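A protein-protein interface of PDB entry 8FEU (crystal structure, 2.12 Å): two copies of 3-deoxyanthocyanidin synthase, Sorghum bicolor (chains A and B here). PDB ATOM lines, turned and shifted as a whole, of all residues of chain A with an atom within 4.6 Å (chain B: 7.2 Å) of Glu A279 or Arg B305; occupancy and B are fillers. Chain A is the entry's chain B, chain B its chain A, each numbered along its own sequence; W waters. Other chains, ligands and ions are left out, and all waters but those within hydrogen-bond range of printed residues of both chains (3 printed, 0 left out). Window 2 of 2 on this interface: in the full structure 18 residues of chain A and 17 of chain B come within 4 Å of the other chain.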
ATOM      1  N   TYR A 273     -10.623   5.941 -19.737  1.00  0.00           N
ATOM      2  CA  TYR A 273      -9.842   5.049 -20.584  1.00  0.00           C
ATOM      3  C   TYR A 273      -8.409   5.556 -20.688  1.00  0.00           C
ATOM      4  O   TYR A 273      -8.183   6.738 -20.978  1.00  0.00           O
ATOM      5  CB  TYR A 273     -10.459   4.931 -21.992  1.00  0.00           C
ATOM      6  CG  TYR A 273     -10.029   3.668 -22.683  1.00  0.00           C
ATOM      7  CD1 TYR A 273      -8.836   3.616 -23.385  1.00  0.00           C
ATOM      8  CD2 TYR A 273     -10.799   2.504 -22.592  1.00  0.00           C
ATOM      9  CE1 TYR A 273      -8.411   2.439 -23.997  1.00  0.00           C
ATOM     10  CE2 TYR A 273     -10.384   1.310 -23.207  1.00  0.00           C
ATOM     11  CZ  TYR A 273      -9.193   1.296 -23.906  1.00  0.00           C
ATOM     12  OH  TYR A 273      -8.754   0.149 -24.501  1.00  0.00           O
ATOM     13  N   PRO A 275      -5.219   4.541 -22.612  1.00  0.00           N
ATOM     14  CA  PRO A 275      -4.407   3.826 -23.595  1.00  0.00           C
ATOM     15  C   PRO A 275      -2.980   4.362 -23.622  1.00  0.00           C
ATOM     16  O   PRO A 275      -2.708   5.512 -23.263  1.00  0.00           O
ATOM     17  CB  PRO A 275      -5.126   4.147 -24.906  1.00  0.00           C
ATOM     18  CG  PRO A 275      -5.609   5.593 -24.680  1.00  0.00           C
ATOM     19  CD  PRO A 275      -5.836   5.752 -23.187  1.00  0.00           C
ATOM     20  N   THR A 276      -2.064   3.495 -24.044  1.00  0.00           N
ATOM     21  CA  THR A 276      -0.788   3.977 -24.554  1.00  0.00           C
ATOM     22  C   THR A 276      -1.008   4.704 -25.876  1.00  0.00           C
ATOM     23  O   THR A 276      -2.052   4.561 -26.527  1.00  0.00           O
ATOM     24  CB  THR A 276       0.188   2.822 -24.772  1.00  0.00           C
ATOM     25  OG1 THR A 276      -0.315   1.980 -25.826  1.00  0.00           O
ATOM     26  CG2 THR A 276       0.367   1.999 -23.495  1.00  0.00           C
ATOM     27  N   LEU A 277       0.007   5.467 -26.301  1.00  0.00           N
ATOM     28  CA  LEU A 277      -0.114   6.169 -27.576  1.00  0.00           C
ATOM     29  C   LEU A 277      -0.214   5.173 -28.729  1.00  0.00           C
ATOM     30  O   LEU A 277      -0.958   5.396 -29.692  1.00  0.00           O
ATOM     31  CB  LEU A 277       1.062   7.129 -27.780  1.00  0.00           C
ATOM     32  CG  LEU A 277       1.057   8.316 -26.800  1.00  0.00           C
ATOM     33  CD1 LEU A 277       2.091   9.381 -27.173  1.00  0.00           C
ATOM     34  CD2 LEU A 277      -0.339   8.947 -26.725  1.00  0.00           C
ATOM     35  N   VAL A 278       0.514   4.054 -28.644  1.00  0.00           N
ATOM     36  CA  VAL A 278       0.465   3.088 -29.735  1.00  0.00           C
ATOM     37  C   VAL A 278      -0.911   2.426 -29.812  1.00  0.00           C
ATOM     38  O   VAL A 278      -1.423   2.177 -30.908  1.00  0.00           O
ATOM     39  CB  VAL A 278       1.605   2.062 -29.605  1.00  0.00           C
ATOM     40  CG1 VAL A 278       1.373   1.134 -28.420  1.00  0.00           C
ATOM     41  CG2 VAL A 278       1.726   1.261 -30.903  1.00  0.00           C
ATOM     42  N   GLU A 279      -1.541   2.142 -28.665  1.00  0.00           N
ATOM     43  CA  GLU A 279      -2.927   1.676 -28.703  1.00  0.00           C
ATOM     44  C   GLU A 279      -3.839   2.731 -29.315  1.00  0.00           C
ATOM     45  O   GLU A 279      -4.644   2.439 -30.204  1.00  0.00           O
ATOM     46  CB  GLU A 279      -3.436   1.303 -27.307  1.00  0.00           C
ATOM     47  CG  GLU A 279      -4.909   0.855 -27.352  1.00  0.00           C
ATOM     48  CD  GLU A 279      -5.539   0.617 -25.993  1.00  0.00           C
ATOM     49  OE1 GLU A 279      -4.844   0.725 -24.963  1.00  0.00           O
ATOM     50  OE2 GLU A 279      -6.756   0.318 -25.963  1.00  0.00           O
ATOM     51  N   LEU A 280      -3.719   3.974 -28.855  1.00  0.00           N
ATOM     52  CA  LEU A 280      -4.555   5.036 -29.397  1.00  0.00           C
ATOM     53  C   LEU A 280      -4.333   5.184 -30.902  1.00  0.00           C
ATOM     54  O   LEU A 280      -5.290   5.244 -31.685  1.00  0.00           O
ATOM     55  CB  LEU A 280      -4.261   6.345 -28.668  1.00  0.00           C
ATOM     56  CG  LEU A 280      -4.964   7.558 -29.250  1.00  0.00           C
ATOM     57  CD1 LEU A 280      -6.463   7.293 -29.274  1.00  0.00           C
ATOM     58  CD2 LEU A 280      -4.646   8.803 -28.426  1.00  0.00           C
ATOM     59  N   ALA A 281      -3.066   5.214 -31.327  1.00  0.00           N
ATOM     60  CA  ALA A 281      -2.772   5.365 -32.749  1.00  0.00           C
ATOM     61  C   ALA A 281      -3.317   4.191 -33.554  1.00  0.00           C
ATOM     62  O   ALA A 281      -3.881   4.380 -34.640  1.00  0.00           O
ATOM     63  CB  ALA A 281      -1.265   5.516 -32.963  1.00  0.00           C
ATOM     64  N   THR A 282      -3.159   2.969 -33.043  1.00  0.00           N
ATOM     65  CA  THR A 282      -3.653   1.806 -33.777  1.00  0.00           C
ATOM     66  C   THR A 282      -5.162   1.887 -33.975  1.00  0.00           C
ATOM     67  O   THR A 282      -5.669   1.645 -35.077  1.00  0.00           O
ATOM     68  CB  THR A 282      -3.269   0.519 -33.044  1.00  0.00           C
ATOM     69  OG1 THR A 282      -1.848   0.462 -32.908  1.00  0.00           O
ATOM     70  CG2 THR A 282      -3.745  -0.720 -33.825  1.00  0.00           C
ATOM     71  N   PHE A 283      -5.899   2.242 -32.923  1.00  0.00           N
ATOM     72  CA  PHE A 283      -7.338   2.393 -33.076  1.00  0.00           C
ATOM     73  C   PHE A 283      -7.663   3.455 -34.122  1.00  0.00           C
ATOM     74  O   PHE A 283      -8.516   3.244 -34.994  1.00  0.00           O
ATOM     75  CB  PHE A 283      -7.983   2.740 -31.733  1.00  0.00           C
ATOM     76  CG  PHE A 283      -9.312   3.416 -31.875  1.00  0.00           C
ATOM     77  CD1 PHE A 283     -10.431   2.676 -32.234  1.00  0.00           C
ATOM     78  CD2 PHE A 283      -9.435   4.785 -31.709  1.00  0.00           C
ATOM     79  CE1 PHE A 283     -11.670   3.304 -32.382  1.00  0.00           C
ATOM     80  CE2 PHE A 283     -10.646   5.413 -31.863  1.00  0.00           C
ATOM     81  CZ  PHE A 283     -11.769   4.676 -32.201  1.00  0.00           C
ATOM     82  N   LEU A 325     -12.604   2.655 -25.962  1.00  0.00           N
ATOM     83  CA  LEU A 325     -11.882   3.718 -26.655  1.00  0.00           C
ATOM     84  C   LEU A 325     -12.721   4.266 -27.804  1.00  0.00           C
ATOM     85  O   LEU A 325     -12.799   5.486 -28.015  1.00  0.00           O
ATOM     86  CB  LEU A 325     -10.516   3.209 -27.148  1.00  0.00           C
ATOM     87  CG  LEU A 325      -9.629   4.256 -27.830  1.00  0.00           C
ATOM     88  CD1 LEU A 325      -9.495   5.546 -26.969  1.00  0.00           C
ATOM     89  CD2 LEU A 325      -8.250   3.678 -28.162  1.00  0.00           C
ATOM     90  N   GLY B 147     -14.288  -7.322 -33.973  1.00  0.00           N
ATOM     91  CA  GLY B 147     -13.349  -6.251 -34.207  1.00  0.00           C
ATOM     92  C   GLY B 147     -13.505  -5.022 -33.329  1.00  0.00           C
ATOM     93  O   GLY B 147     -12.687  -4.104 -33.439  1.00  0.00           O
ATOM     94  N   HIS B 148     -14.520  -4.952 -32.478  1.00  0.00           N
ATOM     95  CA  HIS B 148     -14.635  -3.828 -31.561  1.00  0.00           C
ATOM     96  C   HIS B 148     -14.162  -4.207 -30.162  1.00  0.00           C
ATOM     97  O   HIS B 148     -14.010  -5.385 -29.817  1.00  0.00           O
ATOM     98  CB  HIS B 148     -16.071  -3.304 -31.494  1.00  0.00           C
ATOM     99  CG  HIS B 148     -16.594  -2.849 -32.818  1.00  0.00           C
ATOM    100  ND1 HIS B 148     -16.523  -1.537 -33.235  1.00  0.00           N
ATOM    101  CD2 HIS B 148     -17.159  -3.541 -33.839  1.00  0.00           C
ATOM    102  CE1 HIS B 148     -17.036  -1.438 -34.449  1.00  0.00           C
ATOM    103  NE2 HIS B 148     -17.429  -2.639 -34.837  1.00  0.00           N
ATOM    104  N   GLY B 149     -13.902  -3.167 -29.355  1.00  0.00           N
ATOM    105  CA  GLY B 149     -13.677  -3.373 -27.946  1.00  0.00           C
ATOM    106  C   GLY B 149     -14.984  -3.606 -27.210  1.00  0.00           C
ATOM    107  O   GLY B 149     -16.061  -3.226 -27.654  1.00  0.00           O
ATOM    108  N   HIS B 150     -14.882  -4.241 -26.050  1.00  0.00           N
ATOM    109  CA  HIS B 150     -16.056  -4.498 -25.237  1.00  0.00           C
ATOM    110  C   HIS B 150     -15.646  -4.485 -23.779  1.00  0.00           C
ATOM    111  O   HIS B 150     -14.562  -4.960 -23.441  1.00  0.00           O
ATOM    112  CB  HIS B 150     -16.693  -5.851 -25.594  1.00  0.00           C
ATOM    113  CG  HIS B 150     -17.074  -5.959 -27.036  1.00  0.00           C
ATOM    114  ND1 HIS B 150     -18.256  -5.452 -27.530  1.00  0.00           N
ATOM    115  CD2 HIS B 150     -16.402  -6.457 -28.102  1.00  0.00           C
ATOM    116  CE1 HIS B 150     -18.307  -5.652 -28.834  1.00  0.00           C
ATOM    117  NE2 HIS B 150     -17.194  -6.261 -29.206  1.00  0.00           N
ATOM    118  N   VAL B 151     -16.523  -3.956 -22.928  1.00  0.00           N
ATOM    119  CA  VAL B 151     -16.420  -4.110 -21.482  1.00  0.00           C
ATOM    120  C   VAL B 151     -17.478  -5.134 -21.080  1.00  0.00           C
ATOM    121  O   VAL B 151     -18.667  -4.831 -21.064  1.00  0.00           O
ATOM    122  CB  VAL B 151     -16.614  -2.784 -20.736  1.00  0.00           C
ATOM    123  CG1 VAL B 151     -16.285  -2.973 -19.239  1.00  0.00           C
ATOM    124  CG2 VAL B 151     -15.724  -1.697 -21.339  1.00  0.00           C
ATOM    125  N   LEU B 152     -17.049  -6.338 -20.734  1.00  0.00           N
ATOM    126  CA  LEU B 152     -17.965  -7.358 -20.251  1.00  0.00           C
ATOM    127  C   LEU B 152     -18.200  -7.178 -18.756  1.00  0.00           C
ATOM    128  O   LEU B 152     -17.275  -6.850 -18.005  1.00  0.00           O
ATOM    129  CB  LEU B 152     -17.385  -8.739 -20.530  1.00  0.00           C
ATOM    130  CG  LEU B 152     -17.098  -9.066 -22.009  1.00  0.00           C
ATOM    131  CD1 LEU B 152     -16.597 -10.514 -22.178  1.00  0.00           C
ATOM    132  CD2 LEU B 152     -18.340  -8.834 -22.859  1.00  0.00           C
ATOM    133  N   GLN B 237      -4.432 -13.193 -24.319  1.00  0.00           N
ATOM    134  CA  GLN B 237      -4.157 -11.910 -24.956  1.00  0.00           C
ATOM    135  C   GLN B 237      -4.647 -11.876 -26.411  1.00  0.00           C
ATOM    136  O   GLN B 237      -5.151 -10.844 -26.875  1.00  0.00           O
ATOM    137  CB  GLN B 237      -2.668 -11.607 -24.895  1.00  0.00           C
ATOM    138  CG  GLN B 237      -2.275 -10.580 -25.920  1.00  0.00           C
ATOM    139  CD  GLN B 237      -1.336  -9.569 -25.358  1.00  0.00           C
ATOM    140  OE1 GLN B 237      -1.546  -9.048 -24.238  1.00  0.00           O
ATOM    141  NE2 GLN B 237      -0.250  -9.314 -26.092  1.00  0.00           N
ATOM    142  N   THR B 239      -7.191 -13.268 -27.597  1.00  0.00           N
ATOM    143  CA  THR B 239      -8.630 -13.082 -27.502  1.00  0.00           C
ATOM    144  C   THR B 239      -8.998 -11.690 -26.991  1.00  0.00           C
ATOM    145  O   THR B 239      -9.821 -10.995 -27.601  1.00  0.00           O
ATOM    146  CB  THR B 239      -9.204 -14.153 -26.585  1.00  0.00           C
ATOM    147  OG1 THR B 239      -8.840 -15.441 -27.092  1.00  0.00           O
ATOM    148  CG2 THR B 239     -10.709 -14.032 -26.504  1.00  0.00           C
ATOM    149  N   SER B 240      -8.398 -11.269 -25.870  1.00  0.00           N
ATOM    150  CA  SER B 240      -8.804 -10.050 -25.184  1.00  0.00           C
ATOM    151  C   SER B 240      -7.947  -8.833 -25.494  1.00  0.00           C
ATOM    152  O   SER B 240      -8.382  -7.714 -25.210  1.00  0.00           O
ATOM    153  CB  SER B 240      -8.796 -10.259 -23.662  1.00  0.00           C
ATOM    154  OG  SER B 240      -9.807 -11.169 -23.276  1.00  0.00           O
ATOM    155  N   GLY B 241      -6.745  -9.008 -26.039  1.00  0.00           N
ATOM    156  CA  GLY B 241      -5.856  -7.875 -26.214  1.00  0.00           C
ATOM    157  C   GLY B 241      -5.075  -7.498 -24.972  1.00  0.00           C
ATOM    158  O   GLY B 241      -4.359  -6.491 -24.987  1.00  0.00           O
ATOM    159  N   GLU B 242      -5.173  -8.299 -23.915  1.00  0.00           N
ATOM    160  CA  GLU B 242      -4.619  -8.049 -22.588  1.00  0.00           C
ATOM    161  C   GLU B 242      -4.855  -9.324 -21.776  1.00  0.00           C
ATOM    162  O   GLU B 242      -5.557 -10.236 -22.226  1.00  0.00           O
ATOM    163  CB  GLU B 242      -5.306  -6.821 -21.937  1.00  0.00           C
ATOM    164  CG  GLU B 242      -6.752  -7.132 -21.542  1.00  0.00           C
ATOM    165  CD  GLU B 242      -7.546  -5.946 -21.008  1.00  0.00           C
ATOM    166  OE1 GLU B 242      -7.185  -4.772 -21.259  1.00  0.00           O
ATOM    167  OE2 GLU B 242      -8.544  -6.212 -20.292  1.00  0.00           O
ATOM    168  N   VAL B 243      -4.248  -9.398 -20.589  1.00  0.00           N
ATOM    169  CA  VAL B 243      -4.655 -10.373 -19.584  1.00  0.00           C
ATOM    170  C   VAL B 243      -5.177  -9.591 -18.387  1.00  0.00           C
ATOM    171  O   VAL B 243      -5.093  -8.363 -18.335  1.00  0.00           O
ATOM    172  CB  VAL B 243      -3.533 -11.347 -19.161  1.00  0.00           C
ATOM    173  CG1 VAL B 243      -2.930 -12.083 -20.374  1.00  0.00           C
ATOM    174  CG2 VAL B 243      -2.415 -10.616 -18.388  1.00  0.00           C
ATOM    175  N   HIS B 274      -4.783  -4.988 -15.627  1.00  0.00           N
ATOM    176  CA  HIS B 274      -5.018  -5.553 -16.963  1.00  0.00           C
ATOM    177  C   HIS B 274      -3.876  -5.213 -17.919  1.00  0.00           C
ATOM    178  O   HIS B 274      -4.043  -4.380 -18.818  1.00  0.00           O
ATOM    179  CB  HIS B 274      -6.323  -5.050 -17.580  1.00  0.00           C
ATOM    180  CG  HIS B 274      -7.547  -5.322 -16.764  1.00  0.00           C
ATOM    181  ND1 HIS B 274      -8.770  -4.764 -17.073  1.00  0.00           N
ATOM    182  CD2 HIS B 274      -7.743  -6.064 -15.646  1.00  0.00           C
ATOM    183  CE1 HIS B 274      -9.668  -5.151 -16.183  1.00  0.00           C
ATOM    184  NE2 HIS B 274      -9.071  -5.941 -15.306  1.00  0.00           N
ATOM    185  N   PRO B 275      -2.726  -5.866 -17.792  1.00  0.00           N
ATOM    186  CA  PRO B 275      -1.591  -5.567 -18.677  1.00  0.00           C
ATOM    187  C   PRO B 275      -1.618  -6.375 -19.965  1.00  0.00           C
ATOM    188  O   PRO B 275      -2.116  -7.504 -20.013  1.00  0.00           O
ATOM    189  CB  PRO B 275      -0.390  -6.013 -17.838  1.00  0.00           C
ATOM    190  CG  PRO B 275      -0.936  -7.244 -17.132  1.00  0.00           C
ATOM    191  CD  PRO B 275      -2.447  -7.028 -16.931  1.00  0.00           C
ATOM    192  N   THR B 276      -1.021  -5.798 -21.009  1.00  0.00           N
ATOM    193  CA  THR B 276      -0.537  -6.613 -22.115  1.00  0.00           C
ATOM    194  C   THR B 276       0.616  -7.489 -21.641  1.00  0.00           C
ATOM    195  O   THR B 276       1.272  -7.210 -20.628  1.00  0.00           O
ATOM    196  CB  THR B 276      -0.034  -5.749 -23.273  1.00  0.00           C
ATOM    197  OG1 THR B 276       1.081  -4.956 -22.832  1.00  0.00           O
ATOM    198  CG2 THR B 276      -1.137  -4.794 -23.780  1.00  0.00           C
ATOM    199  N   GLU B 301       0.858  -6.932 -32.030  1.00  0.00           N
ATOM    200  CA  GLU B 301       0.038  -5.835 -32.512  1.00  0.00           C
ATOM    201  C   GLU B 301      -1.055  -5.515 -31.497  1.00  0.00           C
ATOM    202  O   GLU B 301      -1.550  -6.390 -30.780  1.00  0.00           O
ATOM    203  CB  GLU B 301      -0.586  -6.196 -33.862  1.00  0.00           C
ATOM    204  CG  GLU B 301      -1.507  -7.408 -33.788  1.00  0.00           C
ATOM    205  CD  GLU B 301      -2.221  -7.692 -35.092  1.00  0.00           C
ATOM    206  OE1 GLU B 301      -1.540  -7.742 -36.141  1.00  0.00           O
ATOM    207  OE2 GLU B 301      -3.461  -7.872 -35.062  1.00  0.00           O
ATOM    208  N   GLU B 302      -1.434  -4.243 -31.443  1.00  0.00           N
ATOM    209  CA  GLU B 302      -2.525  -3.835 -30.574  1.00  0.00           C
ATOM    210  C   GLU B 302      -3.834  -4.405 -31.100  1.00  0.00           C
ATOM    211  O   GLU B 302      -4.130  -4.289 -32.291  1.00  0.00           O
ATOM    212  CB  GLU B 302      -2.594  -2.314 -30.501  1.00  0.00           C
ATOM    213  CG  GLU B 302      -1.328  -1.666 -29.946  1.00  0.00           C
ATOM    214  CD  GLU B 302      -1.126  -1.935 -28.460  1.00  0.00           C
ATOM    215  OE1 GLU B 302      -2.124  -2.077 -27.718  1.00  0.00           O
ATOM    216  OE2 GLU B 302       0.044  -1.995 -28.028  1.00  0.00           O
ATOM    217  N   ARG B 303      -4.607  -5.033 -30.219  1.00  0.00           N
ATOM    218  CA  ARG B 303      -5.904  -5.615 -30.543  1.00  0.00           C
ATOM    219  C   ARG B 303      -7.013  -4.876 -29.803  1.00  0.00           C
ATOM    220  O   ARG B 303      -6.776  -4.272 -28.754  1.00  0.00           O
ATOM    221  CB  ARG B 303      -5.954  -7.102 -30.155  1.00  0.00           C
ATOM    222  CG  ARG B 303      -5.044  -8.009 -30.982  1.00  0.00           C
ATOM    223  CD  ARG B 303      -4.676  -9.300 -30.232  1.00  0.00           C
ATOM    224  NE  ARG B 303      -3.504  -9.934 -30.824  1.00  0.00           N
ATOM    225  CZ  ARG B 303      -3.504 -10.543 -32.003  1.00  0.00           C
ATOM    226  NH1 ARG B 303      -4.624 -10.718 -32.691  1.00  0.00           N
ATOM    227  NH2 ARG B 303      -2.353 -10.984 -32.504  1.00  0.00           N
ATOM    228  N   PRO B 304      -8.244  -4.921 -30.303  1.00  0.00           N
ATOM    229  CA  PRO B 304      -9.352  -4.336 -29.544  1.00  0.00           C
ATOM    230  C   PRO B 304      -9.441  -5.013 -28.186  1.00  0.00           C
ATOM    231  O   PRO B 304      -9.178  -6.211 -28.051  1.00  0.00           O
ATOM    232  CB  PRO B 304     -10.582  -4.635 -30.409  1.00  0.00           C
ATOM    233  CG  PRO B 304     -10.023  -4.910 -31.788  1.00  0.00           C
ATOM    234  CD  PRO B 304      -8.718  -5.610 -31.513  1.00  0.00           C
ATOM    235  N   ARG B 305      -9.791  -4.228 -27.171  1.00  0.00           N
ATOM    236  CA  ARG B 305      -9.812  -4.704 -25.792  1.00  0.00           C
ATOM    237  C   ARG B 305     -11.171  -5.310 -25.469  1.00  0.00           C
ATOM    238  O   ARG B 305     -12.198  -4.627 -25.537  1.00  0.00           O
ATOM    239  CB  ARG B 305      -9.494  -3.560 -24.828  1.00  0.00           C
ATOM    240  CG  ARG B 305      -8.119  -2.975 -25.003  1.00  0.00           C
ATOM    241  CD  ARG B 305      -7.111  -4.082 -25.249  1.00  0.00           C
ATOM    242  NE  ARG B 305      -5.798  -3.539 -25.580  1.00  0.00           N
ATOM    243  CZ  ARG B 305      -4.934  -3.075 -24.686  1.00  0.00           C
ATOM    244  NH1 ARG B 305      -5.226  -3.056 -23.387  1.00  0.00           N
ATOM    245  NH2 ARG B 305      -3.753  -2.614 -25.104  1.00  0.00           N
ATOM    246  N   VAL B 306     -11.175  -6.583 -25.123  1.00  0.00           N
ATOM    247  CA  VAL B 306     -12.331  -7.235 -24.530  1.00  0.00           C
ATOM    248  C   VAL B 306     -11.985  -7.438 -23.064  1.00  0.00           C
ATOM    249  O   VAL B 306     -11.286  -8.392 -22.711  1.00  0.00           O
ATOM    250  CB  VAL B 306     -12.677  -8.559 -25.223  1.00  0.00           C
ATOM    251  CG1 VAL B 306     -13.856  -9.201 -24.521  1.00  0.00           C
ATOM    252  CG2 VAL B 306     -13.004  -8.323 -26.691  1.00  0.00           C
ATOM    253  N   THR B 307     -12.454  -6.531 -22.213  1.00  0.00           N
ATOM    254  CA  THR B 307     -11.964  -6.442 -20.848  1.00  0.00           C
ATOM    255  C   THR B 307     -13.117  -6.661 -19.874  1.00  0.00           C
ATOM    256  O   THR B 307     -14.286  -6.599 -20.247  1.00  0.00           O
ATOM    257  CB  THR B 307     -11.271  -5.064 -20.614  1.00  0.00           C
ATOM    258  OG1 THR B 307     -10.623  -5.064 -19.351  1.00  0.00           O
ATOM    259  CG2 THR B 307     -12.305  -3.925 -20.656  1.00  0.00           C
HETATM  260  O   HOH W   1      -5.869   0.082 -22.362  1.00  0.00           O
HETATM  261  O   HOH W   2      -2.562   0.406 -24.027  1.00  0.00           O
HETATM  262  O   HOH W   3      -0.537  -0.824 -25.174  1.00  0.00           O
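Of the 22 printed residues of chain B, 2 touch a printed residue of chain A. Printed residues of chain B that touch a printed residue of chain A: Glu B302 and Arg B305. Along chain B the printed residues that touch a printed residue of chain A span positions 302 to 305. Hydrophobic or aromatic side chains of chain A that line the printed part of chain B: Tyr A273 and Val A278. Among the printed residues, 5 pairs touch across the chains. Among the printed residues, Asp or Glu carboxylates within 4 Å of a Lys or Arg side-chain nitrogen of the other chain: Glu A279 with Arg B305 (3.5 Å).
NH2 of Arg B305 lies within salt-bridge range of OE1 of Glu A279 (3.5 Å).
OE1 of Glu B302 is in salt-bridge range of NH2 of Arg B305 (3.1 Å). The guanidinium group (NH1) of Arg B305 is in salt-bridge range of the side-chain carboxylate (OE1) of Glu B242, 3.4 Å away. The backbone NH (N) of His B150 is in hydrogen-bond range of the backbone carbonyl oxygen (O) of Arg B305 (2.8 Å). OG1 of Thr A276 lies within hydrogen-bond range of N of Glu A279. The side-chain hydroxyl of Thr A282 is in hydrogen-bond range of the backbone carbonyl oxygen of Val A278. O of Arg B303 sits at hydrogen-bond distance from NE of Arg B305, 3.4 Å away.
Among the printed residues, pairs that only touch across the chains: Tyr A273 with Arg B305 (3.2 Å), Val A278 with Glu B302 (3.4 Å), Glu A279 with Glu B302 (3.6 Å) and Thr A282 with Glu B302 (3.7 Å).
Printed residues of chain B within 4 Å of Val A278: Glu B302. Of the printed residues of chain B, Thr A282 touches Glu B302 (3.7 Å). Printed residues of chain A within 4 Å of Glu B302: Val A278, Glu A279 and Thr A282.
2 positions are printed for both chains.
Water W2 lies within hydrogen-bond range of the side-chain carboxylate of Glu A279, the backbone NH of Thr A276 and the guanidinium group of Arg B305. Water W1 bridges OE1 of Glu A279 (2.9 Å) and NH1 of Arg B305 (3.4 Å). Water W3 bridges OG1 of Thr A276 and OE2 of Glu B302.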
